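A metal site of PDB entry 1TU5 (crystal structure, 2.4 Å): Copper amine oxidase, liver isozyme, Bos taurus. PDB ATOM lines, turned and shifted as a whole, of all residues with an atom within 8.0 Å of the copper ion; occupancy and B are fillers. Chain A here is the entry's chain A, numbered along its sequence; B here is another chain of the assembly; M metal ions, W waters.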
ATOM      1  N   ALA A 353     -18.224 -19.656   3.897  1.00  0.00           N
ATOM      2  CA  ALA A 353     -19.550 -19.949   4.403  1.00  0.00           C
ATOM      3  C   ALA A 353     -19.567 -19.663   5.911  1.00  0.00           C
ATOM      4  O   ALA A 353     -18.687 -20.105   6.635  1.00  0.00           O
ATOM      5  CB  ALA A 353     -19.849 -21.407   4.152  1.00  0.00           C
ATOM      6  N   TYR A 355     -21.825 -20.094   9.282  1.00  0.00           N
ATOM      7  CA  TYR A 355     -22.963 -20.839   9.821  1.00  0.00           C
ATOM      8  C   TYR A 355     -23.556 -20.343  11.118  1.00  0.00           C
ATOM      9  O   TYR A 355     -22.920 -19.589  11.870  1.00  0.00           O
ATOM     10  CB  TYR A 355     -22.605 -22.316  10.054  1.00  0.00           C
ATOM     11  CG  TYR A 355     -22.665 -23.172   8.829  1.00  0.00           C
ATOM     12  CD1 TYR A 355     -21.610 -23.192   7.922  1.00  0.00           C
ATOM     13  CD2 TYR A 355     -23.808 -23.923   8.523  1.00  0.00           C
ATOM     14  CE1 TYR A 355     -21.680 -23.921   6.737  1.00  0.00           C
ATOM     15  CE2 TYR A 355     -23.900 -24.645   7.341  1.00  0.00           C
ATOM     16  CZ  TYR A 355     -22.827 -24.637   6.462  1.00  0.00           C
ATOM     17  OH  TYR A 355     -22.895 -25.352   5.297  1.00  0.00           O
ATOM     18  N   ASN A 453     -19.469 -31.238   1.671  1.00  0.00           N
ATOM     19  CA  ASN A 453     -20.831 -31.411   1.173  1.00  0.00           C
ATOM     20  C   ASN A 453     -21.206 -30.492  -0.020  1.00  0.00           C
ATOM     21  O   ASN A 453     -22.061 -30.836  -0.831  1.00  0.00           O
ATOM     22  CB  ASN A 453     -21.840 -31.212   2.315  1.00  0.00           C
ATOM     23  CG  ASN A 453     -21.704 -29.857   2.976  1.00  0.00           C
ATOM     24  OD1 ASN A 453     -20.691 -29.549   3.600  1.00  0.00           O
ATOM     25  ND2 ASN A 453     -22.742 -29.037   2.830  1.00  0.00           N
ATOM     26  N   TPQ A 454     -20.549 -29.333  -0.137  1.00  0.00           N
ATOM     27  CA  TPQ A 454     -20.873 -28.428  -1.245  1.00  0.00           C
ATOM     28  CB  TPQ A 454     -20.536 -26.969  -0.908  1.00  0.00           C
ATOM     29  C   TPQ A 454     -20.130 -28.734  -2.549  1.00  0.00           C
ATOM     30  O   TPQ A 454     -19.021 -29.271  -2.543  1.00  0.00           O
ATOM     31  C1  TPQ A 454     -20.551 -26.592   0.549  1.00  0.00           C
ATOM     32  C2  TPQ A 454     -21.751 -26.524   1.230  1.00  0.00           C
ATOM     33  O2  TPQ A 454     -22.886 -26.782   0.598  1.00  0.00           O
ATOM     34  C3  TPQ A 454     -21.758 -26.140   2.566  1.00  0.00           C
ATOM     35  C4  TPQ A 454     -20.565 -25.840   3.211  1.00  0.00           C
ATOM     36  O4  TPQ A 454     -20.574 -25.456   4.527  1.00  0.00           O
ATOM     37  C5  TPQ A 454     -19.373 -25.915   2.521  1.00  0.00           C
ATOM     38  O5  TPQ A 454     -18.227 -25.600   3.131  1.00  0.00           O
ATOM     39  C6  TPQ A 454     -19.358 -26.291   1.205  1.00  0.00           C
ATOM     40  N   TYR A 456     -19.101 -26.514  -5.922  1.00  0.00           N
ATOM     41  CA  TYR A 456     -19.087 -25.138  -6.405  1.00  0.00           C
ATOM     42  C   TYR A 456     -18.667 -25.183  -7.867  1.00  0.00           C
ATOM     43  O   TYR A 456     -17.538 -25.574  -8.146  1.00  0.00           O
ATOM     44  CB  TYR A 456     -18.068 -24.257  -5.654  1.00  0.00           C
ATOM     45  CG  TYR A 456     -18.429 -23.866  -4.250  1.00  0.00           C
ATOM     46  CD1 TYR A 456     -17.661 -24.298  -3.173  1.00  0.00           C
ATOM     47  CD2 TYR A 456     -19.545 -23.079  -3.985  1.00  0.00           C
ATOM     48  CE1 TYR A 456     -17.996 -23.957  -1.852  1.00  0.00           C
ATOM     49  CE2 TYR A 456     -19.894 -22.724  -2.663  1.00  0.00           C
ATOM     50  CZ  TYR A 456     -19.114 -23.170  -1.607  1.00  0.00           C
ATOM     51  OH  TYR A 456     -19.451 -22.829  -0.306  1.00  0.00           O
ATOM     52  N   ALA A 474     -23.809 -22.798  -6.630  1.00  0.00           N
ATOM     53  CA  ALA A 474     -23.661 -23.760  -5.563  1.00  0.00           C
ATOM     54  C   ALA A 474     -24.683 -24.891  -5.668  1.00  0.00           C
ATOM     55  O   ALA A 474     -25.872 -24.666  -5.885  1.00  0.00           O
ATOM     56  CB  ALA A 474     -23.786 -23.058  -4.207  1.00  0.00           C
ATOM     57  N   THR A 475     -24.201 -26.121  -5.541  1.00  0.00           N
ATOM     58  CA  THR A 475     -25.086 -27.274  -5.620  1.00  0.00           C
ATOM     59  C   THR A 475     -24.514 -28.314  -4.649  1.00  0.00           C
ATOM     60  O   THR A 475     -23.574 -28.034  -3.906  1.00  0.00           O
ATOM     61  CB  THR A 475     -25.154 -27.806  -7.058  1.00  0.00           C
ATOM     62  OG1 THR A 475     -26.161 -28.825  -7.155  1.00  0.00           O
ATOM     63  CG2 THR A 475     -23.834 -28.375  -7.476  1.00  0.00           C
ATOM     64  N   TYR A 477     -25.107 -31.008  -1.380  1.00  0.00           N
ATOM     65  CA  TYR A 477     -25.936 -31.382  -0.223  1.00  0.00           C
ATOM     66  C   TYR A 477     -25.721 -30.406   0.924  1.00  0.00           C
ATOM     67  O   TYR A 477     -24.621 -29.897   1.095  1.00  0.00           O
ATOM     68  CB  TYR A 477     -25.519 -32.744   0.304  1.00  0.00           C
ATOM     69  CG  TYR A 477     -25.499 -33.854  -0.697  1.00  0.00           C
ATOM     70  CD1 TYR A 477     -24.584 -34.893  -0.576  1.00  0.00           C
ATOM     71  CD2 TYR A 477     -26.439 -33.923  -1.712  1.00  0.00           C
ATOM     72  CE1 TYR A 477     -24.615 -35.994  -1.461  1.00  0.00           C
ATOM     73  CE2 TYR A 477     -26.485 -35.011  -2.595  1.00  0.00           C
ATOM     74  CZ  TYR A 477     -25.569 -36.050  -2.465  1.00  0.00           C
ATOM     75  OH  TYR A 477     -25.619 -37.130  -3.328  1.00  0.00           O
ATOM     76  N   ILE A 478     -26.734 -30.196   1.755  1.00  0.00           N
ATOM     77  CA  ILE A 478     -26.575 -29.304   2.899  1.00  0.00           C
ATOM     78  C   ILE A 478     -26.061 -30.075   4.126  1.00  0.00           C
ATOM     79  O   ILE A 478     -26.331 -31.276   4.273  1.00  0.00           O
ATOM     80  CB  ILE A 478     -27.933 -28.601   3.301  1.00  0.00           C
ATOM     81  CG1 ILE A 478     -28.949 -29.630   3.788  1.00  0.00           C
ATOM     82  CG2 ILE A 478     -28.505 -27.824   2.130  1.00  0.00           C
ATOM     83  CD1 ILE A 478     -30.288 -29.048   4.158  1.00  0.00           C
ATOM     84  N   SER A 479     -25.305 -29.411   5.007  1.00  0.00           N
ATOM     85  CA  SER A 479     -24.865 -30.097   6.211  1.00  0.00           C
ATOM     86  C   SER A 479     -25.995 -29.864   7.215  1.00  0.00           C
ATOM     87  O   SER A 479     -26.483 -28.752   7.361  1.00  0.00           O
ATOM     88  CB  SER A 479     -23.563 -29.493   6.742  1.00  0.00           C
ATOM     89  OG  SER A 479     -23.825 -28.279   7.406  1.00  0.00           O
ATOM     90  N   PRO A 501     -29.314 -25.799   9.062  1.00  0.00           N
ATOM     91  CA  PRO A 501     -28.797 -24.516   9.562  1.00  0.00           C
ATOM     92  C   PRO A 501     -28.463 -23.398   8.614  1.00  0.00           C
ATOM     93  O   PRO A 501     -27.922 -23.645   7.552  1.00  0.00           O
ATOM     94  CB  PRO A 501     -27.571 -24.949  10.389  1.00  0.00           C
ATOM     95  CG  PRO A 501     -27.043 -26.072   9.616  1.00  0.00           C
ATOM     96  CD  PRO A 501     -28.275 -26.838   9.139  1.00  0.00           C
ATOM     97  N   VAL A 502     -28.782 -22.172   9.012  1.00  0.00           N
ATOM     98  CA  VAL A 502     -28.503 -20.982   8.211  1.00  0.00           C
ATOM     99  C   VAL A 502     -27.025 -20.815   7.931  1.00  0.00           C
ATOM    100  O   VAL A 502     -26.162 -21.142   8.766  1.00  0.00           O
ATOM    101  CB  VAL A 502     -28.802 -19.627   8.928  1.00  0.00           C
ATOM    102  CG1 VAL A 502     -29.756 -18.826   8.109  1.00  0.00           C
ATOM    103  CG2 VAL A 502     -29.212 -19.837  10.361  1.00  0.00           C
ATOM    104  N   HIS A 503     -26.734 -20.214   6.790  1.00  0.00           N
ATOM    105  CA  HIS A 503     -25.373 -19.885   6.411  1.00  0.00           C
ATOM    106  C   HIS A 503     -25.387 -18.945   5.210  1.00  0.00           C
ATOM    107  O   HIS A 503     -26.376 -18.822   4.470  1.00  0.00           O
ATOM    108  CB  HIS A 503     -24.548 -21.153   6.090  1.00  0.00           C
ATOM    109  CG  HIS A 503     -25.171 -22.050   5.066  1.00  0.00           C
ATOM    110  ND1 HIS A 503     -26.319 -22.776   5.304  1.00  0.00           N
ATOM    111  CD2 HIS A 503     -24.810 -22.313   3.782  1.00  0.00           C
ATOM    112  CE1 HIS A 503     -26.636 -23.448   4.206  1.00  0.00           C
ATOM    113  NE2 HIS A 503     -25.747 -23.193   3.274  1.00  0.00           N
ATOM    114  N   THR A 504     -24.293 -18.225   5.058  1.00  0.00           N
ATOM    115  CA  THR A 504     -24.127 -17.341   3.939  1.00  0.00           C
ATOM    116  C   THR A 504     -23.079 -18.033   3.037  1.00  0.00           C
ATOM    117  O   THR A 504     -22.318 -18.879   3.514  1.00  0.00           O
ATOM    118  CB  THR A 504     -23.578 -15.966   4.405  1.00  0.00           C
ATOM    119  OG1 THR A 504     -22.393 -16.153   5.184  1.00  0.00           O
ATOM    120  CG2 THR A 504     -24.604 -15.218   5.243  1.00  0.00           C
ATOM    121  N   HIS A 505     -23.089 -17.730   1.739  1.00  0.00           N
ATOM    122  CA  HIS A 505     -22.086 -18.267   0.811  1.00  0.00           C
ATOM    123  C   HIS A 505     -21.466 -17.027   0.214  1.00  0.00           C
ATOM    124  O   HIS A 505     -22.170 -16.138  -0.260  1.00  0.00           O
ATOM    125  CB  HIS A 505     -22.711 -19.059  -0.304  1.00  0.00           C
ATOM    126  CG  HIS A 505     -23.084 -20.457   0.076  1.00  0.00           C
ATOM    127  ND1 HIS A 505     -22.159 -21.467   0.165  1.00  0.00           N
ATOM    128  CD2 HIS A 505     -24.287 -21.013   0.339  1.00  0.00           C
ATOM    129  CE1 HIS A 505     -22.783 -22.597   0.460  1.00  0.00           C
ATOM    130  NE2 HIS A 505     -24.071 -22.348   0.576  1.00  0.00           N
ATOM    131  N   PHE A 665     -24.679 -15.019  -1.196  1.00  0.00           N
ATOM    132  CA  PHE A 665     -26.106 -15.010  -0.903  1.00  0.00           C
ATOM    133  C   PHE A 665     -26.381 -15.673   0.458  1.00  0.00           C
ATOM    134  O   PHE A 665     -25.522 -16.320   1.054  1.00  0.00           O
ATOM    135  CB  PHE A 665     -26.890 -15.703  -2.042  1.00  0.00           C
ATOM    136  CG  PHE A 665     -26.541 -17.161  -2.231  1.00  0.00           C
ATOM    137  CD1 PHE A 665     -27.320 -18.161  -1.659  1.00  0.00           C
ATOM    138  CD2 PHE A 665     -25.433 -17.527  -2.970  1.00  0.00           C
ATOM    139  CE1 PHE A 665     -26.991 -19.513  -1.826  1.00  0.00           C
ATOM    140  CE2 PHE A 665     -25.090 -18.878  -3.139  1.00  0.00           C
ATOM    141  CZ  PHE A 665     -25.883 -19.864  -2.566  1.00  0.00           C
ATOM    142  N   LEU A 666     -27.578 -15.485   0.966  1.00  0.00           N
ATOM    143  CA  LEU A 666     -27.970 -16.085   2.229  1.00  0.00           C
ATOM    144  C   LEU A 666     -28.657 -17.381   1.868  1.00  0.00           C
ATOM    145  O   LEU A 666     -29.429 -17.444   0.905  1.00  0.00           O
ATOM    146  CB  LEU A 666     -28.994 -15.196   2.956  1.00  0.00           C
ATOM    147  CG  LEU A 666     -29.165 -15.236   4.483  1.00  0.00           C
ATOM    148  CD1 LEU A 666     -30.628 -14.971   4.838  1.00  0.00           C
ATOM    149  CD2 LEU A 666     -28.663 -16.533   5.071  1.00  0.00           C
ATOM    150  N   HIS A 667     -28.417 -18.409   2.664  1.00  0.00           N
ATOM    151  CA  HIS A 667     -29.069 -19.683   2.430  1.00  0.00           C
ATOM    152  C   HIS A 667     -29.728 -20.169   3.720  1.00  0.00           C
ATOM    153  O   HIS A 667     -29.037 -20.538   4.674  1.00  0.00           O
ATOM    154  CB  HIS A 667     -28.051 -20.747   1.986  1.00  0.00           C
ATOM    155  CG  HIS A 667     -28.685 -22.043   1.589  1.00  0.00           C
ATOM    156  ND1 HIS A 667     -27.952 -23.086   1.065  1.00  0.00           N
ATOM    157  CD2 HIS A 667     -29.977 -22.432   1.548  1.00  0.00           C
ATOM    158  CE1 HIS A 667     -28.773 -24.064   0.716  1.00  0.00           C
ATOM    159  NE2 HIS A 667     -30.015 -23.687   0.997  1.00  0.00           N
ATOM    160  N   ILE A 668     -31.063 -20.169   3.742  1.00  0.00           N
ATOM    161  CA  ILE A 668     -31.811 -20.698   4.871  1.00  0.00           C
ATOM    162  C   ILE A 668     -32.318 -21.989   4.259  1.00  0.00           C
ATOM    163  O   ILE A 668     -33.190 -21.980   3.417  1.00  0.00           O
ATOM    164  CB  ILE A 668     -33.010 -19.811   5.285  1.00  0.00           C
ATOM    165  CG1 ILE A 668     -32.500 -18.416   5.714  1.00  0.00           C
ATOM    166  CG2 ILE A 668     -33.712 -20.433   6.510  1.00  0.00           C
ATOM    167  CD1 ILE A 668     -33.586 -17.417   5.994  1.00  0.00           C
ATOM    168  N   PRO A 669     -31.743 -23.125   4.658  1.00  0.00           N
ATOM    169  CA  PRO A 669     -32.213 -24.366   4.062  1.00  0.00           C
ATOM    170  C   PRO A 669     -33.719 -24.577   4.214  1.00  0.00           C
ATOM    171  O   PRO A 669     -34.339 -24.146   5.203  1.00  0.00           O
ATOM    172  CB  PRO A 669     -31.391 -25.444   4.786  1.00  0.00           C
ATOM    173  CG  PRO A 669     -30.191 -24.748   5.227  1.00  0.00           C
ATOM    174  CD  PRO A 669     -30.705 -23.395   5.665  1.00  0.00           C
ATOM    175  N   ASP A 673     -34.493 -28.390  -0.406  1.00  0.00           N
ATOM    176  CA  ASP A 673     -33.075 -28.701  -0.434  1.00  0.00           C
ATOM    177  C   ASP A 673     -32.755 -30.178  -0.157  1.00  0.00           C
ATOM    178  O   ASP A 673     -31.585 -30.581  -0.189  1.00  0.00           O
ATOM    179  CB  ASP A 673     -32.309 -27.889   0.605  1.00  0.00           C
ATOM    180  CG  ASP A 673     -32.195 -26.442   0.252  1.00  0.00           C
ATOM    181  OD1 ASP A 673     -32.081 -26.138  -0.949  1.00  0.00           O
ATOM    182  OD2 ASP A 673     -32.202 -25.622   1.183  1.00  0.00           O
ATOM    183  N   THR A 677     -29.610 -29.731  -3.080  1.00  0.00           N
ATOM    184  CA  THR A 677     -29.986 -28.369  -3.481  1.00  0.00           C
ATOM    185  C   THR A 677     -29.615 -28.152  -4.940  1.00  0.00           C
ATOM    186  O   THR A 677     -28.585 -28.636  -5.409  1.00  0.00           O
ATOM    187  CB  THR A 677     -29.328 -27.281  -2.593  1.00  0.00           C
ATOM    188  OG1 THR A 677     -27.914 -27.283  -2.804  1.00  0.00           O
ATOM    189  CG2 THR A 677     -29.530 -27.583  -1.151  1.00  0.00           C
ATOM    190  N   TYR B 569     -35.463 -12.871   2.354  1.00  0.00           N
ATOM    191  CA  TYR B 569     -36.398 -13.955   2.068  1.00  0.00           C
ATOM    192  C   TYR B 569     -37.806 -13.451   2.266  1.00  0.00           C
ATOM    193  O   TYR B 569     -38.260 -13.323   3.400  1.00  0.00           O
ATOM    194  CB  TYR B 569     -36.170 -15.137   3.017  1.00  0.00           C
ATOM    195  CG  TYR B 569     -35.141 -16.116   2.542  1.00  0.00           C
ATOM    196  CD1 TYR B 569     -35.523 -17.370   2.098  1.00  0.00           C
ATOM    197  CD2 TYR B 569     -33.778 -15.791   2.515  1.00  0.00           C
ATOM    198  CE1 TYR B 569     -34.600 -18.272   1.633  1.00  0.00           C
ATOM    199  CE2 TYR B 569     -32.834 -16.700   2.038  1.00  0.00           C
ATOM    200  CZ  TYR B 569     -33.266 -17.947   1.599  1.00  0.00           C
ATOM    201  OH  TYR B 569     -32.391 -18.863   1.079  1.00  0.00           O
HETATM  202 CU    CU M   1     -25.917 -23.327   1.081  1.00  0.00          CU
HETATM  203  O   HOH W   1     -25.631 -24.963  -1.484  1.00  0.00           O
HETATM  204  O   HOH W   2     -25.379 -25.752   1.150  1.00  0.00           O
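The copper ion is bound by ND1 of His 667 (2.0 Å), NE2 of His 505 (2.1 Å), NE2 of His 503 (2.2 Å) and water W2 (2.5 Å).
Of the 23 residues printed, 3 come within 4 Å of the copper ion.
NE2 of His 667 lies within hydrogen-bond range of OD2 of Asp 673, 2.9 Å away.
N of His 505 sits at hydrogen-bond distance from O of Phe 665 (2.9 Å).
A ring nitrogen (ND1) of His 505 lies within hydrogen-bond range of the side-chain hydroxyl (OH) of Tyr 456 (3.1 Å).
A ring nitrogen (ND1) of His 503 is in hydrogen-bond range of the backbone carbonyl oxygen (O) of Pro 501, at 2.9 Å.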
